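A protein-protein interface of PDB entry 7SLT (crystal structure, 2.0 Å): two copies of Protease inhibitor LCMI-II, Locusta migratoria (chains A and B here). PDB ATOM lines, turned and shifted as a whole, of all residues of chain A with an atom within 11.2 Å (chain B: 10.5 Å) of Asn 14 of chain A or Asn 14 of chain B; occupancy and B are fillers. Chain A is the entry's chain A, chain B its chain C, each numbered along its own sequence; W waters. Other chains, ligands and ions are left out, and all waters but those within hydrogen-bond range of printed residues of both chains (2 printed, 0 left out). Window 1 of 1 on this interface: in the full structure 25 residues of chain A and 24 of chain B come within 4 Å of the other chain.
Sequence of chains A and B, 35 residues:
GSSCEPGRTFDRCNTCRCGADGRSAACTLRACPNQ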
ATOM      1  N   ARG A   8      -7.424  16.281  -8.699  1.00  0.00           N
ATOM      2  CA  ARG A   8      -6.800  17.631  -8.575  1.00  0.00           C
ATOM      3  C   ARG A   8      -5.360  17.609  -9.109  1.00  0.00           C
ATOM      4  O   ARG A   8      -4.632  16.593  -8.897  1.00  0.00           O
ATOM      5  CB  ARG A   8      -6.751  18.123  -7.125  1.00  0.00           C
ATOM      6  CG  ARG A   8      -8.051  18.728  -6.606  1.00  0.00           C
ATOM      7  CD  ARG A   8      -9.218  18.607  -7.559  1.00  0.00           C
ATOM      8  N   THR A   9      -4.942  18.716  -9.712  1.00  0.00           N
ATOM      9  CA  THR A   9      -3.533  18.959 -10.122  1.00  0.00           C
ATOM     10  C   THR A   9      -2.821  19.626  -8.953  1.00  0.00           C
ATOM     11  O   THR A   9      -3.479  20.355  -8.193  1.00  0.00           O
ATOM     12  CB  THR A   9      -3.435  19.769 -11.421  1.00  0.00           C
ATOM     13  OG1 THR A   9      -3.929  21.079 -11.165  1.00  0.00           O
ATOM     14  CG2 THR A   9      -4.213  19.132 -12.544  1.00  0.00           C
ATOM     15  N   PHE A  10      -1.537  19.337  -8.777  1.00  0.00           N
ATOM     16  CA  PHE A  10      -0.690  19.942  -7.722  1.00  0.00           C
ATOM     17  C   PHE A  10       0.761  19.995  -8.226  1.00  0.00           C
ATOM     18  O   PHE A  10       1.133  19.238  -9.157  1.00  0.00           O
ATOM     19  CB  PHE A  10      -0.817  19.146  -6.416  1.00  0.00           C
ATOM     20  CG  PHE A  10      -0.321  17.719  -6.504  1.00  0.00           C
ATOM     21  CD1 PHE A  10      -1.137  16.700  -6.975  1.00  0.00           C
ATOM     22  CD2 PHE A  10       0.952  17.389  -6.070  1.00  0.00           C
ATOM     23  CE1 PHE A  10      -0.676  15.393  -7.055  1.00  0.00           C
ATOM     24  CE2 PHE A  10       1.415  16.088  -6.157  1.00  0.00           C
ATOM     25  CZ  PHE A  10       0.602  15.094  -6.645  1.00  0.00           C
ATOM     26  N   ASP A  11       1.532  20.917  -7.656  1.00  0.00           N
ATOM     27  CA  ASP A  11       2.919  21.245  -8.067  1.00  0.00           C
ATOM     28  C   ASP A  11       3.860  20.549  -7.087  1.00  0.00           C
ATOM     29  O   ASP A  11       3.525  20.436  -5.908  1.00  0.00           O
ATOM     30  CB  ASP A  11       3.158  22.758  -8.156  1.00  0.00           C
ATOM     31  CG  ASP A  11       2.520  23.410  -9.378  1.00  0.00           C
ATOM     32  OD1 ASP A  11       2.178  22.674 -10.325  1.00  0.00           O
ATOM     33  OD2 ASP A  11       2.372  24.654  -9.380  1.00  0.00           O
ATOM     34  N   ARG A  12       4.945  20.003  -7.604  1.00  0.00           N
ATOM     35  CA  ARG A  12       5.932  19.279  -6.812  1.00  0.00           C
ATOM     36  C   ARG A  12       7.276  19.661  -7.383  1.00  0.00           C
ATOM     37  O   ARG A  12       7.477  19.440  -8.569  1.00  0.00           O
ATOM     38  CB  ARG A  12       5.738  17.768  -6.881  1.00  0.00           C
ATOM     39  CG  ARG A  12       6.488  17.001  -5.813  1.00  0.00           C
ATOM     40  CD  ARG A  12       5.536  16.736  -4.677  1.00  0.00           C
ATOM     41  NE  ARG A  12       6.078  15.755  -3.758  1.00  0.00           N
ATOM     42  CZ  ARG A  12       5.949  15.789  -2.436  1.00  0.00           C
ATOM     43  NH1 ARG A  12       6.482  14.809  -1.732  1.00  0.00           N
ATOM     44  NH2 ARG A  12       5.301  16.781  -1.826  1.00  0.00           N
ATOM     45  N   CYS A  13       8.164  20.158  -6.529  1.00  0.00           N
ATOM     46  CA  CYS A  13       9.503  20.658  -6.929  1.00  0.00           C
ATOM     47  C   CYS A  13      10.589  19.919  -6.149  1.00  0.00           C
ATOM     48  O   CYS A  13      10.329  19.480  -5.001  1.00  0.00           O
ATOM     49  CB  CYS A  13       9.578  22.170  -6.771  1.00  0.00           C
ATOM     50  SG  CYS A  13       8.339  22.997  -7.803  1.00  0.00           S
ATOM     51  N   ASN A  14      11.736  19.739  -6.802  1.00  0.00           N
ATOM     52  CA  ASN A  14      12.831  18.861  -6.334  1.00  0.00           C
ATOM     53  C   ASN A  14      14.134  19.616  -6.545  1.00  0.00           C
ATOM     54  O   ASN A  14      14.203  20.451  -7.457  1.00  0.00           O
ATOM     55  CB  ASN A  14      12.943  17.524  -7.087  1.00  0.00           C
ATOM     56  CG  ASN A  14      11.624  16.823  -7.364  1.00  0.00           C
ATOM     57  OD1 ASN A  14      11.370  16.408  -8.492  1.00  0.00           O
ATOM     58  ND2 ASN A  14      10.781  16.655  -6.353  1.00  0.00           N
ATOM     59  N   THR A  15      15.151  19.250  -5.789  1.00  0.00           N
ATOM     60  CA  THR A  15      16.527  19.655  -6.069  1.00  0.00           C
ATOM     61  C   THR A  15      17.359  18.377  -6.091  1.00  0.00           C
ATOM     62  O   THR A  15      17.187  17.533  -5.221  1.00  0.00           O
ATOM     63  CB  THR A  15      16.975  20.753  -5.103  1.00  0.00           C
ATOM     64  OG1 THR A  15      18.255  21.119  -5.594  1.00  0.00           O
ATOM     65  CG2 THR A  15      17.050  20.331  -3.654  1.00  0.00           C
ATOM     66  N   CYS A  16      18.178  18.243  -7.109  1.00  0.00           N
ATOM     67  CA  CYS A  16      18.882  16.981  -7.448  1.00  0.00           C
ATOM     68  C   CYS A  16      20.373  17.279  -7.600  1.00  0.00           C
ATOM     69  O   CYS A  16      20.723  18.384  -8.062  1.00  0.00           O
ATOM     70  CB  CYS A  16      18.302  16.390  -8.724  1.00  0.00           C
ATOM     71  SG  CYS A  16      16.550  15.964  -8.563  1.00  0.00           S
ATOM     72  N   ARG A  17      21.215  16.316  -7.262  1.00  0.00           N
ATOM     73  CA  ARG A  17      22.567  16.208  -7.846  1.00  0.00           C
ATOM     74  C   ARG A  17      22.669  14.910  -8.653  1.00  0.00           C
ATOM     75  O   ARG A  17      22.323  13.828  -8.144  1.00  0.00           O
ATOM     76  CB  ARG A  17      23.644  16.283  -6.762  1.00  0.00           C
ATOM     77  CG  ARG A  17      25.025  16.542  -7.332  1.00  0.00           C
ATOM     78  CD  ARG A  17      26.021  16.713  -6.197  1.00  0.00           C
ATOM     79  NE  ARG A  17      25.789  17.957  -5.476  1.00  0.00           N
ATOM     80  CZ  ARG A  17      26.156  19.149  -5.922  1.00  0.00           C
ATOM     81  NH1 ARG A  17      26.775  19.268  -7.084  1.00  0.00           N
ATOM     82  NH2 ARG A  17      25.932  20.226  -5.194  1.00  0.00           N
ATOM     83  N   CYS A  18      23.172  15.040  -9.870  1.00  0.00           N
ATOM     84  CA  CYS A  18      23.344  13.965 -10.869  1.00  0.00           C
ATOM     85  C   CYS A  18      24.504  13.047 -10.481  1.00  0.00           C
ATOM     86  O   CYS A  18      25.588  13.555 -10.118  1.00  0.00           O
ATOM     87  CB  CYS A  18      23.566  14.640 -12.201  1.00  0.00           C
ATOM     88  SG  CYS A  18      23.612  13.508 -13.596  1.00  0.00           S
ATOM     89  N   ALA A  25      20.202  10.418 -10.128  1.00  0.00           N
ATOM     90  CA  ALA A  25      20.432  11.638  -9.326  1.00  0.00           C
ATOM     91  C   ALA A  25      19.920  11.393  -7.912  1.00  0.00           C
ATOM     92  O   ALA A  25      19.044  10.564  -7.763  1.00  0.00           O
ATOM     93  CB  ALA A  25      19.754  12.791 -10.009  1.00  0.00           C
ATOM     94  N   ALA A  26      20.487  12.081  -6.928  1.00  0.00           N
ATOM     95  CA  ALA A  26      19.995  12.095  -5.543  1.00  0.00           C
ATOM     96  C   ALA A  26      19.234  13.398  -5.384  1.00  0.00           C
ATOM     97  O   ALA A  26      19.809  14.425  -5.694  1.00  0.00           O
ATOM     98  CB  ALA A  26      21.162  11.959  -4.589  1.00  0.00           C
ATOM     99  N   CYS A  27      17.953  13.331  -5.019  1.00  0.00           N
ATOM    100  CA  CYS A  27      17.036  14.482  -5.009  1.00  0.00           C
ATOM    101  C   CYS A  27      16.341  14.586  -3.669  1.00  0.00           C
ATOM    102  O   CYS A  27      16.209  13.584  -2.934  1.00  0.00           O
ATOM    103  CB  CYS A  27      15.927  14.383  -6.052  1.00  0.00           C
ATOM    104  SG  CYS A  27      16.529  14.120  -7.739  1.00  0.00           S
ATOM    105  N   THR A  28      15.918  15.801  -3.382  1.00  0.00           N
ATOM    106  CA  THR A  28      15.072  16.092  -2.220  1.00  0.00           C
ATOM    107  C   THR A  28      14.008  17.105  -2.618  1.00  0.00           C
ATOM    108  O   THR A  28      14.187  17.877  -3.598  1.00  0.00           O
ATOM    109  CB  THR A  28      15.944  16.508  -1.037  1.00  0.00           C
ATOM    110  OG1 THR A  28      15.120  16.138   0.061  1.00  0.00           O
ATOM    111  CG2 THR A  28      16.335  17.968  -1.048  1.00  0.00           C
ATOM    112  N   LEU A  29      12.948  17.095  -1.821  1.00  0.00           N
ATOM    113  CA  LEU A  29      11.788  18.006  -1.956  1.00  0.00           C
ATOM    114  C   LEU A  29      12.239  19.445  -1.691  1.00  0.00           C
ATOM    115  O   LEU A  29      13.130  19.638  -0.883  1.00  0.00           O
ATOM    116  CB  LEU A  29      10.702  17.542  -0.983  1.00  0.00           C
ATOM    117  CG  LEU A  29       9.281  17.911  -1.382  1.00  0.00           C
ATOM    118  CD1 LEU A  29       8.927  17.307  -2.740  1.00  0.00           C
ATOM    119  CD2 LEU A  29       8.299  17.457  -0.309  1.00  0.00           C
ATOM    120  N   ARG A  30      11.724  20.397  -2.460  1.00  0.00           N
ATOM    121  CA  ARG A  30      11.862  21.834  -2.162  1.00  0.00           C
ATOM    122  C   ARG A  30      10.541  22.531  -2.497  1.00  0.00           C
ATOM    123  O   ARG A  30       9.708  21.958  -3.262  1.00  0.00           O
ATOM    124  CB  ARG A  30      13.045  22.448  -2.913  1.00  0.00           C
ATOM    125  CG  ARG A  30      12.829  22.601  -4.405  1.00  0.00           C
ATOM    126  CD  ARG A  30      13.937  23.454  -4.983  1.00  0.00           C
ATOM    127  NE  ARG A  30      13.646  24.014  -6.292  1.00  0.00           N
ATOM    128  CZ  ARG A  30      13.050  25.185  -6.521  1.00  0.00           C
ATOM    129  NH1 ARG A  30      12.866  25.586  -7.767  1.00  0.00           N
ATOM    130  NH2 ARG A  30      12.628  25.946  -5.526  1.00  0.00           N
ATOM    131  N   ALA A  31      10.376  23.736  -1.956  1.00  0.00           N
ATOM    132  CA  ALA A  31       9.199  24.596  -2.180  1.00  0.00           C
ATOM    133  C   ALA A  31       9.283  25.118  -3.613  1.00  0.00           C
ATOM    134  O   ALA A  31      10.389  25.454  -4.060  1.00  0.00           O
ATOM    135  CB  ALA A  31       9.159  25.686  -1.138  1.00  0.00           C
ATOM    136  N   CYS A  32       8.165  25.018  -4.336  1.00  0.00           N
ATOM    137  CA  CYS A  32       7.972  25.444  -5.742  1.00  0.00           C
ATOM    138  C   CYS A  32       7.908  26.961  -5.885  1.00  0.00           C
ATOM    139  O   CYS A  32       7.190  27.612  -5.136  1.00  0.00           O
ATOM    140  CB  CYS A  32       6.656  24.883  -6.251  1.00  0.00           C
ATOM    141  SG  CYS A  32       6.775  23.112  -6.554  1.00  0.00           S
ATOM    142  N   PRO A  33       8.575  27.564  -6.896  1.00  0.00           N
ATOM    143  CA  PRO A  33       8.613  29.016  -7.047  1.00  0.00           C
ATOM    144  C   PRO A  33       7.661  29.521  -8.143  1.00  0.00           C
ATOM    145  O   PRO A  33       7.958  29.384  -9.335  1.00  0.00           O
ATOM    146  CB  PRO A  33      10.096  29.199  -7.413  1.00  0.00           C
ATOM    147  CG  PRO A  33      10.473  27.939  -8.190  1.00  0.00           C
ATOM    148  CD  PRO A  33       9.370  26.919  -7.953  1.00  0.00           C
ATOM    149  N   ARG B   8      26.453  17.729 -11.377  1.00  0.00           N
ATOM    150  CA  ARG B   8      25.852  19.082 -11.358  1.00  0.00           C
ATOM    151  C   ARG B   8      24.500  19.011 -10.652  1.00  0.00           C
ATOM    152  O   ARG B   8      23.818  17.969 -10.793  1.00  0.00           O
ATOM    153  CB  ARG B   8      25.757  19.633 -12.783  1.00  0.00           C
ATOM    154  CG  ARG B   8      27.034  20.313 -13.267  1.00  0.00           C
ATOM    155  CD  ARG B   8      26.902  20.903 -14.668  1.00  0.00           C
ATOM    156  NE  ARG B   8      25.858  21.938 -14.769  1.00  0.00           N
ATOM    157  CZ  ARG B   8      26.045  23.265 -14.750  1.00  0.00           C
ATOM    158  NH1 ARG B   8      27.256  23.791 -14.638  1.00  0.00           N
ATOM    159  NH2 ARG B   8      24.997  24.068 -14.846  1.00  0.00           N
ATOM    160  N   THR B   9      24.131  20.058  -9.900  1.00  0.00           N
ATOM    161  CA  THR B   9      22.772  20.181  -9.323  1.00  0.00           C
ATOM    162  C   THR B   9      21.805  20.604 -10.425  1.00  0.00           C
ATOM    163  O   THR B   9      22.230  21.243 -11.418  1.00  0.00           O
ATOM    164  CB  THR B   9      22.665  21.174  -8.160  1.00  0.00           C
ATOM    165  OG1 THR B   9      22.849  22.478  -8.707  1.00  0.00           O
ATOM    166  CG2 THR B   9      23.648  20.914  -7.045  1.00  0.00           C
ATOM    167  N   PHE B  10      20.552  20.202 -10.289  1.00  0.00           N
ATOM    168  CA  PHE B  10      19.432  20.695 -11.115  1.00  0.00           C
ATOM    169  C   PHE B  10      18.162  20.661 -10.272  1.00  0.00           C
ATOM    170  O   PHE B  10      18.046  19.829  -9.367  1.00  0.00           O
ATOM    171  CB  PHE B  10      19.334  19.880 -12.401  1.00  0.00           C
ATOM    172  CG  PHE B  10      19.007  18.416 -12.239  1.00  0.00           C
ATOM    173  CD1 PHE B  10      20.011  17.477 -12.034  1.00  0.00           C
ATOM    174  CD2 PHE B  10      17.706  17.965 -12.380  1.00  0.00           C
ATOM    175  CE1 PHE B  10      19.718  16.123 -11.952  1.00  0.00           C
ATOM    176  CE2 PHE B  10      17.411  16.615 -12.295  1.00  0.00           C
ATOM    177  CZ  PHE B  10      18.420  15.697 -12.070  1.00  0.00           C
ATOM    178  N   ASP B  11      17.237  21.547 -10.599  1.00  0.00           N
ATOM    179  CA  ASP B  11      15.928  21.704  -9.921  1.00  0.00           C
ATOM    180  C   ASP B  11      14.825  21.337 -10.909  1.00  0.00           C
ATOM    181  O   ASP B  11      14.947  21.676 -12.113  1.00  0.00           O
ATOM    182  CB  ASP B  11      15.756  23.123  -9.410  1.00  0.00           C
ATOM    183  CG  ASP B  11      16.611  23.414  -8.184  1.00  0.00           C
ATOM    184  OD1 ASP B  11      17.560  22.658  -7.933  1.00  0.00           O
ATOM    185  OD2 ASP B  11      16.286  24.355  -7.483  1.00  0.00           O
ATOM    186  N   ARG B  12      13.806  20.639 -10.440  1.00  0.00           N
ATOM    187  CA  ARG B  12      12.654  20.275 -11.300  1.00  0.00           C
ATOM    188  C   ARG B  12      11.396  20.912 -10.723  1.00  0.00           C
ATOM    189  O   ARG B  12      11.197  20.858  -9.504  1.00  0.00           O
ATOM    190  CB  ARG B  12      12.476  18.760 -11.454  1.00  0.00           C
ATOM    191  CG  ARG B  12      13.683  18.015 -12.021  1.00  0.00           C
ATOM    192  CD  ARG B  12      14.118  18.387 -13.437  1.00  0.00           C
ATOM    193  NE  ARG B  12      13.278  17.857 -14.512  1.00  0.00           N
ATOM    194  CZ  ARG B  12      13.511  17.996 -15.820  1.00  0.00           C
ATOM    195  NH1 ARG B  12      12.675  17.471 -16.706  1.00  0.00           N
ATOM    196  NH2 ARG B  12      14.570  18.658 -16.245  1.00  0.00           N
ATOM    197  N   CYS B  13      10.541  21.419 -11.601  1.00  0.00           N
ATOM    198  CA  CYS B  13       9.277  22.111 -11.247  1.00  0.00           C
ATOM    199  C   CYS B  13       8.133  21.379 -11.949  1.00  0.00           C
ATOM    200  O   CYS B  13       7.913  21.602 -13.152  1.00  0.00           O
ATOM    201  CB  CYS B  13       9.400  23.588 -11.617  1.00  0.00           C
ATOM    202  SG  CYS B  13      10.427  24.509 -10.442  1.00  0.00           S
ATOM    203  N   ASN B  14       7.523  20.425 -11.249  1.00  0.00           N
ATOM    204  CA  ASN B  14       6.637  19.398 -11.842  1.00  0.00           C
ATOM    205  C   ASN B  14       5.180  19.727 -11.507  1.00  0.00           C
ATOM    206  O   ASN B  14       4.909  20.286 -10.442  1.00  0.00           O
ATOM    207  CB  ASN B  14       6.959  17.991 -11.326  1.00  0.00           C
ATOM    208  CG  ASN B  14       8.411  17.631 -11.542  1.00  0.00           C
ATOM    209  OD1 ASN B  14       9.031  16.962 -10.698  1.00  0.00           O
ATOM    210  ND2 ASN B  14       8.935  18.036 -12.679  1.00  0.00           N
ATOM    211  N   THR B  15       4.268  19.370 -12.392  1.00  0.00           N
ATOM    212  CA  THR B  15       2.819  19.446 -12.113  1.00  0.00           C
ATOM    213  C   THR B  15       2.229  18.056 -12.296  1.00  0.00           C
ATOM    214  O   THR B  15       2.456  17.466 -13.349  1.00  0.00           O
ATOM    215  CB  THR B  15       2.100  20.430 -13.030  1.00  0.00           C
ATOM    216  OG1 THR B  15       2.745  21.695 -12.859  1.00  0.00           O
ATOM    217  CG2 THR B  15       0.630  20.516 -12.681  1.00  0.00           C
ATOM    218  N   CYS B  16       1.562  17.547 -11.271  1.00  0.00           N
ATOM    219  CA  CYS B  16       1.015  16.184 -11.264  1.00  0.00           C
ATOM    220  C   CYS B  16      -0.505  16.240 -11.134  1.00  0.00           C
ATOM    221  O   CYS B  16      -1.023  17.195 -10.550  1.00  0.00           O
ATOM    222  CB  CYS B  16       1.643  15.377 -10.143  1.00  0.00           C
ATOM    223  SG  CYS B  16       3.429  15.206 -10.370  1.00  0.00           S
ATOM    224  N   ARG B  17      -1.141  15.195 -11.633  1.00  0.00           N
ATOM    225  CA  ARG B  17      -2.573  14.879 -11.462  1.00  0.00           C
ATOM    226  C   ARG B  17      -2.698  13.731 -10.464  1.00  0.00           C
ATOM    227  O   ARG B  17      -2.089  12.661 -10.684  1.00  0.00           O
ATOM    228  CB  ARG B  17      -3.162  14.470 -12.812  1.00  0.00           C
ATOM    229  CG  ARG B  17      -4.651  14.177 -12.779  1.00  0.00           C
ATOM    230  CD  ARG B  17      -5.482  15.421 -12.622  1.00  0.00           C
ATOM    231  NE  ARG B  17      -5.338  16.361 -13.741  1.00  0.00           N
ATOM    232  CZ  ARG B  17      -6.261  17.258 -14.072  1.00  0.00           C
ATOM    233  NH1 ARG B  17      -7.378  17.352 -13.359  1.00  0.00           N
ATOM    234  NH2 ARG B  17      -6.058  18.075 -15.088  1.00  0.00           N
ATOM    235  N   SER B  24      -0.073  10.593  -7.006  1.00  0.00           N
ATOM    236  CA  SER B  24       0.003  11.131  -8.391  1.00  0.00           C
ATOM    237  C   SER B  24      -0.215   9.961  -9.362  1.00  0.00           C
ATOM    238  O   SER B  24       0.226   8.841  -9.086  1.00  0.00           O
ATOM    239  CB  SER B  24       1.281  11.873  -8.680  1.00  0.00           C
ATOM    240  OG  SER B  24       2.397  11.013  -8.595  1.00  0.00           O
ATOM    241  N   ALA B  26      -0.291  10.987 -12.974  1.00  0.00           N
ATOM    242  CA  ALA B  26       0.317  11.582 -14.185  1.00  0.00           C
ATOM    243  C   ALA B  26       1.047  12.860 -13.781  1.00  0.00           C
ATOM    244  O   ALA B  26       0.529  13.573 -12.911  1.00  0.00           O
ATOM    245  CB  ALA B  26      -0.750  11.881 -15.194  1.00  0.00           C
ATOM    246  N   CYS B  27       2.197  13.140 -14.394  1.00  0.00           N
ATOM    247  CA  CYS B  27       3.012  14.341 -14.055  1.00  0.00           C
ATOM    248  C   CYS B  27       3.611  14.905 -15.336  1.00  0.00           C
ATOM    249  O   CYS B  27       3.942  14.101 -16.239  1.00  0.00           O
ATOM    250  CB  CYS B  27       4.164  14.032 -13.110  1.00  0.00           C
ATOM    251  SG  CYS B  27       3.680  13.500 -11.454  1.00  0.00           S
ATOM    252  N   THR B  28       3.625  16.230 -15.444  1.00  0.00           N
ATOM    253  CA  THR B  28       4.428  16.972 -16.429  1.00  0.00           C
ATOM    254  C   THR B  28       5.700  17.326 -15.674  1.00  0.00           C
ATOM    255  O   THR B  28       5.560  17.948 -14.612  1.00  0.00           O
ATOM    256  CB  THR B  28       3.677  18.180 -17.018  1.00  0.00           C
ATOM    257  OG1 THR B  28       2.590  17.731 -17.827  1.00  0.00           O
ATOM    258  CG2 THR B  28       4.612  19.026 -17.862  1.00  0.00           C
ATOM    259  N   LEU B  29       6.848  16.813 -16.135  1.00  0.00           N
ATOM    260  CA  LEU B  29       8.160  17.051 -15.518  1.00  0.00           C
ATOM    261  C   LEU B  29       8.764  18.201 -16.316  1.00  0.00           C
ATOM    262  O   LEU B  29       8.608  18.187 -17.580  1.00  0.00           O
ATOM    263  CB  LEU B  29       9.008  15.779 -15.593  1.00  0.00           C
ATOM    264  CG  LEU B  29       8.352  14.497 -15.087  1.00  0.00           C
ATOM    265  CD1 LEU B  29       9.353  13.348 -15.110  1.00  0.00           C
ATOM    266  CD2 LEU B  29       7.765  14.671 -13.699  1.00  0.00           C
ATOM    267  N   ARG B  30       9.294  19.193 -15.614  1.00  0.00           N
ATOM    268  CA  ARG B  30       9.976  20.349 -16.234  1.00  0.00           C
ATOM    269  C   ARG B  30      11.230  20.685 -15.427  1.00  0.00           C
ATOM    270  O   ARG B  30      11.208  20.589 -14.180  1.00  0.00           O
ATOM    271  CB  ARG B  30       9.095  21.598 -16.281  1.00  0.00           C
ATOM    272  CG  ARG B  30       7.618  21.376 -16.527  1.00  0.00           C
ATOM    273  CD  ARG B  30       6.919  22.724 -16.643  1.00  0.00           C
ATOM    274  NE  ARG B  30       5.473  22.605 -16.729  1.00  0.00           N
ATOM    275  CZ  ARG B  30       4.672  22.276 -15.719  1.00  0.00           C
ATOM    276  NH1 ARG B  30       5.158  22.019 -14.512  1.00  0.00           N
ATOM    277  NH2 ARG B  30       3.371  22.171 -15.940  1.00  0.00           N
ATOM    278  N   ALA B  31      12.290  21.102 -16.109  1.00  0.00           N
ATOM    279  CA  ALA B  31      13.399  21.856 -15.486  1.00  0.00           C
ATOM    280  C   ALA B  31      12.769  23.119 -14.909  1.00  0.00           C
ATOM    281  O   ALA B  31      11.751  23.536 -15.471  1.00  0.00           O
ATOM    282  CB  ALA B  31      14.469  22.139 -16.517  1.00  0.00           C
ATOM    283  N   CYS B  32      13.215  23.612 -13.749  1.00  0.00           N
ATOM    284  CA  CYS B  32      12.874  24.975 -13.236  1.00  0.00           C
ATOM    285  C   CYS B  32      13.759  25.990 -13.960  1.00  0.00           C
ATOM    286  O   CYS B  32      14.950  25.745 -14.122  1.00  0.00           O
ATOM    287  CB  CYS B  32      13.132  25.153 -11.746  1.00  0.00           C
ATOM    288  SG  CYS B  32      12.363  23.903 -10.690  1.00  0.00           S
ATOM    289  N   PRO B  33      13.245  27.163 -14.402  1.00  0.00           N
ATOM    290  CA  PRO B  33      14.080  28.144 -15.102  1.00  0.00           C
ATOM    291  C   PRO B  33      14.934  28.969 -14.126  1.00  0.00           C
ATOM    292  O   PRO B  33      15.191  28.529 -12.994  1.00  0.00           O
ATOM    293  CB  PRO B  33      13.055  29.001 -15.871  1.00  0.00           C
ATOM    294  CG  PRO B  33      11.720  28.274 -15.692  1.00  0.00           C
ATOM    295  CD  PRO B  33      11.839  27.591 -14.344  1.00  0.00           C
HETATM  296  O   HOH W   1      11.759  14.923 -10.966  1.00  0.00           O
HETATM  297  O   HOH W   2       6.003  23.364 -10.395  1.00  0.00           O
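The backbone carbonyl oxygen (O) of Phe 10 of chain A sits at hydrogen-bond distance from the backbone NH (N) of Cys 16 of chain B, at 2.7 Å. The side-chain hydroxyl (OG1) of Thr 15 of chain B sits at hydrogen-bond distance from the side-chain carboxylate (OD1) of Asp 11 of chain A (2.8 Å). The backbone NH (N) of Arg 12 of chain A is in hydrogen-bond range of the backbone carbonyl oxygen (O) of Asn 14 of chain B (2.9 Å). The backbone carbonyl oxygen (O) of Arg 12 of chain B lies within hydrogen-bond range of the backbone NH (N) of Asn 14 of chain A (3.0 Å). The side-chain amide oxygen (OD1) of Asn 14 of chain B lies close to the side-chain amide oxygen (OD1) of Asn 14 of chain A (3.3 Å). OG1 of Thr 15 of chain A is in hydrogen-bond range of OD1 of Asp 11 of chain B (2.9 Å). N of Cys 16 of chain A lies within hydrogen-bond range of O of Phe 10 of chain B (2.8 Å). O of Arg 8 of chain B sits at hydrogen-bond distance from N of Cys 18 of chain A, 3.1 Å away. NE of Arg 30 of chain A lies within salt-bridge range of OD2 of Asp 11 of chain B, 2.9 Å away. NH1 of Arg 30 of chain A is in hydrogen-bond range of SG of Cys 13 of chain B (3.8 Å). The guanidinium group (NH1) of Arg 30 of chain A is in hydrogen-bond range of the side-chain sulfur (SG) of Cys 32 of chain B (3.4 Å). SG of Cys 13 of chain A lies close to SG of Cys 13 of chain B (3.7 Å).
The backbone NH (N) of Arg 30 of chain A sits at hydrogen-bond distance from the backbone carbonyl oxygen (O) of Cys 13 of chain A (3.0 Å). NE of Arg 12 of chain B lies close to O of Arg 30 of chain B, 3.4 Å away. The side-chain sulfur (SG) of Cys 13 of chain B forms a disulfide with the side-chain sulfur (SG) of Cys 32 of chain B, 2.0 Å away.
CA of Thr 9 of chain A touches O of Cys 16 of chain B (3.1 Å). Thr 9 of chain A touches Arg 17 of chain B (CG2 to CZ, 3.2 Å). Asn 14 of chain B touches Asp 11 of chain A. Cys 16 of chain A touches Thr 9 of chain B (O to CA, 3.0 Å). CG2 of Thr 9 of chain B touches NH2 of Arg 17 of chain A, 3.0 Å away. Phe 10 of chain B touches Ala 25 of chain A (CZ to CB, 3.8 Å).
Of the 20 printed residues of chain A, 14 touch a printed residue of chain B. Hydrophobic or aromatic side chains of chain A within 4 Å of the printed part of chain B: Phe 10, Ala 25 and Pro 33. Among the printed residues, Asp or Glu carboxylates within 4 Å of a Lys or Arg side-chain nitrogen of the other chain: Arg 30 of chain A with Asp 11 of chain B (2.9 Å).
Water W1 lies within hydrogen-bond range of the side-chain amide oxygen (OD1) of Asn 14 of chain A (2.9 Å) and the side-chain amide oxygen (OD1) of Asn 14 of chain B (3.4 Å). Water W2 lies within hydrogen-bond range of the backbone carbonyl oxygen (O) of Asn 14 of chain B (3.3 Å) and the side-chain sulfur (SG) of Cys 13 of chain A (3.5 Å).
Cys 13 of chain A touches just these residues of chain B: Arg 12 (3.1 Å) and Cys 13 (3.7 Å). Of chain B, only Phe 10 and Asp 11 come within 4 Å of Thr 15 of chain A. Of the printed residues of chain B, Arg 17 of chain A touches Arg 8 (3.7 Å) and Thr 9 (3.0 Å). Of the printed residues of chain B, Cys 18 of chain A touches Arg 8 (3.1 Å). Printed residues of chain A within 4 Å of Cys 13 of chain B: Arg 12 (3.95 Å), Cys 13 (3.7 Å), Arg 30 (3.8 Å) and Pro 33 (3.6 Å). Asn 14 of chain B touches three residues of chain A. No residue of chain A comes within 4 Å of Arg 30 of chain B.
Asp 11 of chain A touches Thr 15 of chain B, and with the chains exchanged Thr 15 of chain A touches Asp 11 of chain B. Arg 30 of chain A touches Cys 32 of chain B, but with the chains exchanged Cys 32 of chain A does not touch Arg 30 of chain B (8.2 Å). Of the 27 pairs that touch across the chains among the printed residues, 20 have their exchanged pair printed and touching as well.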
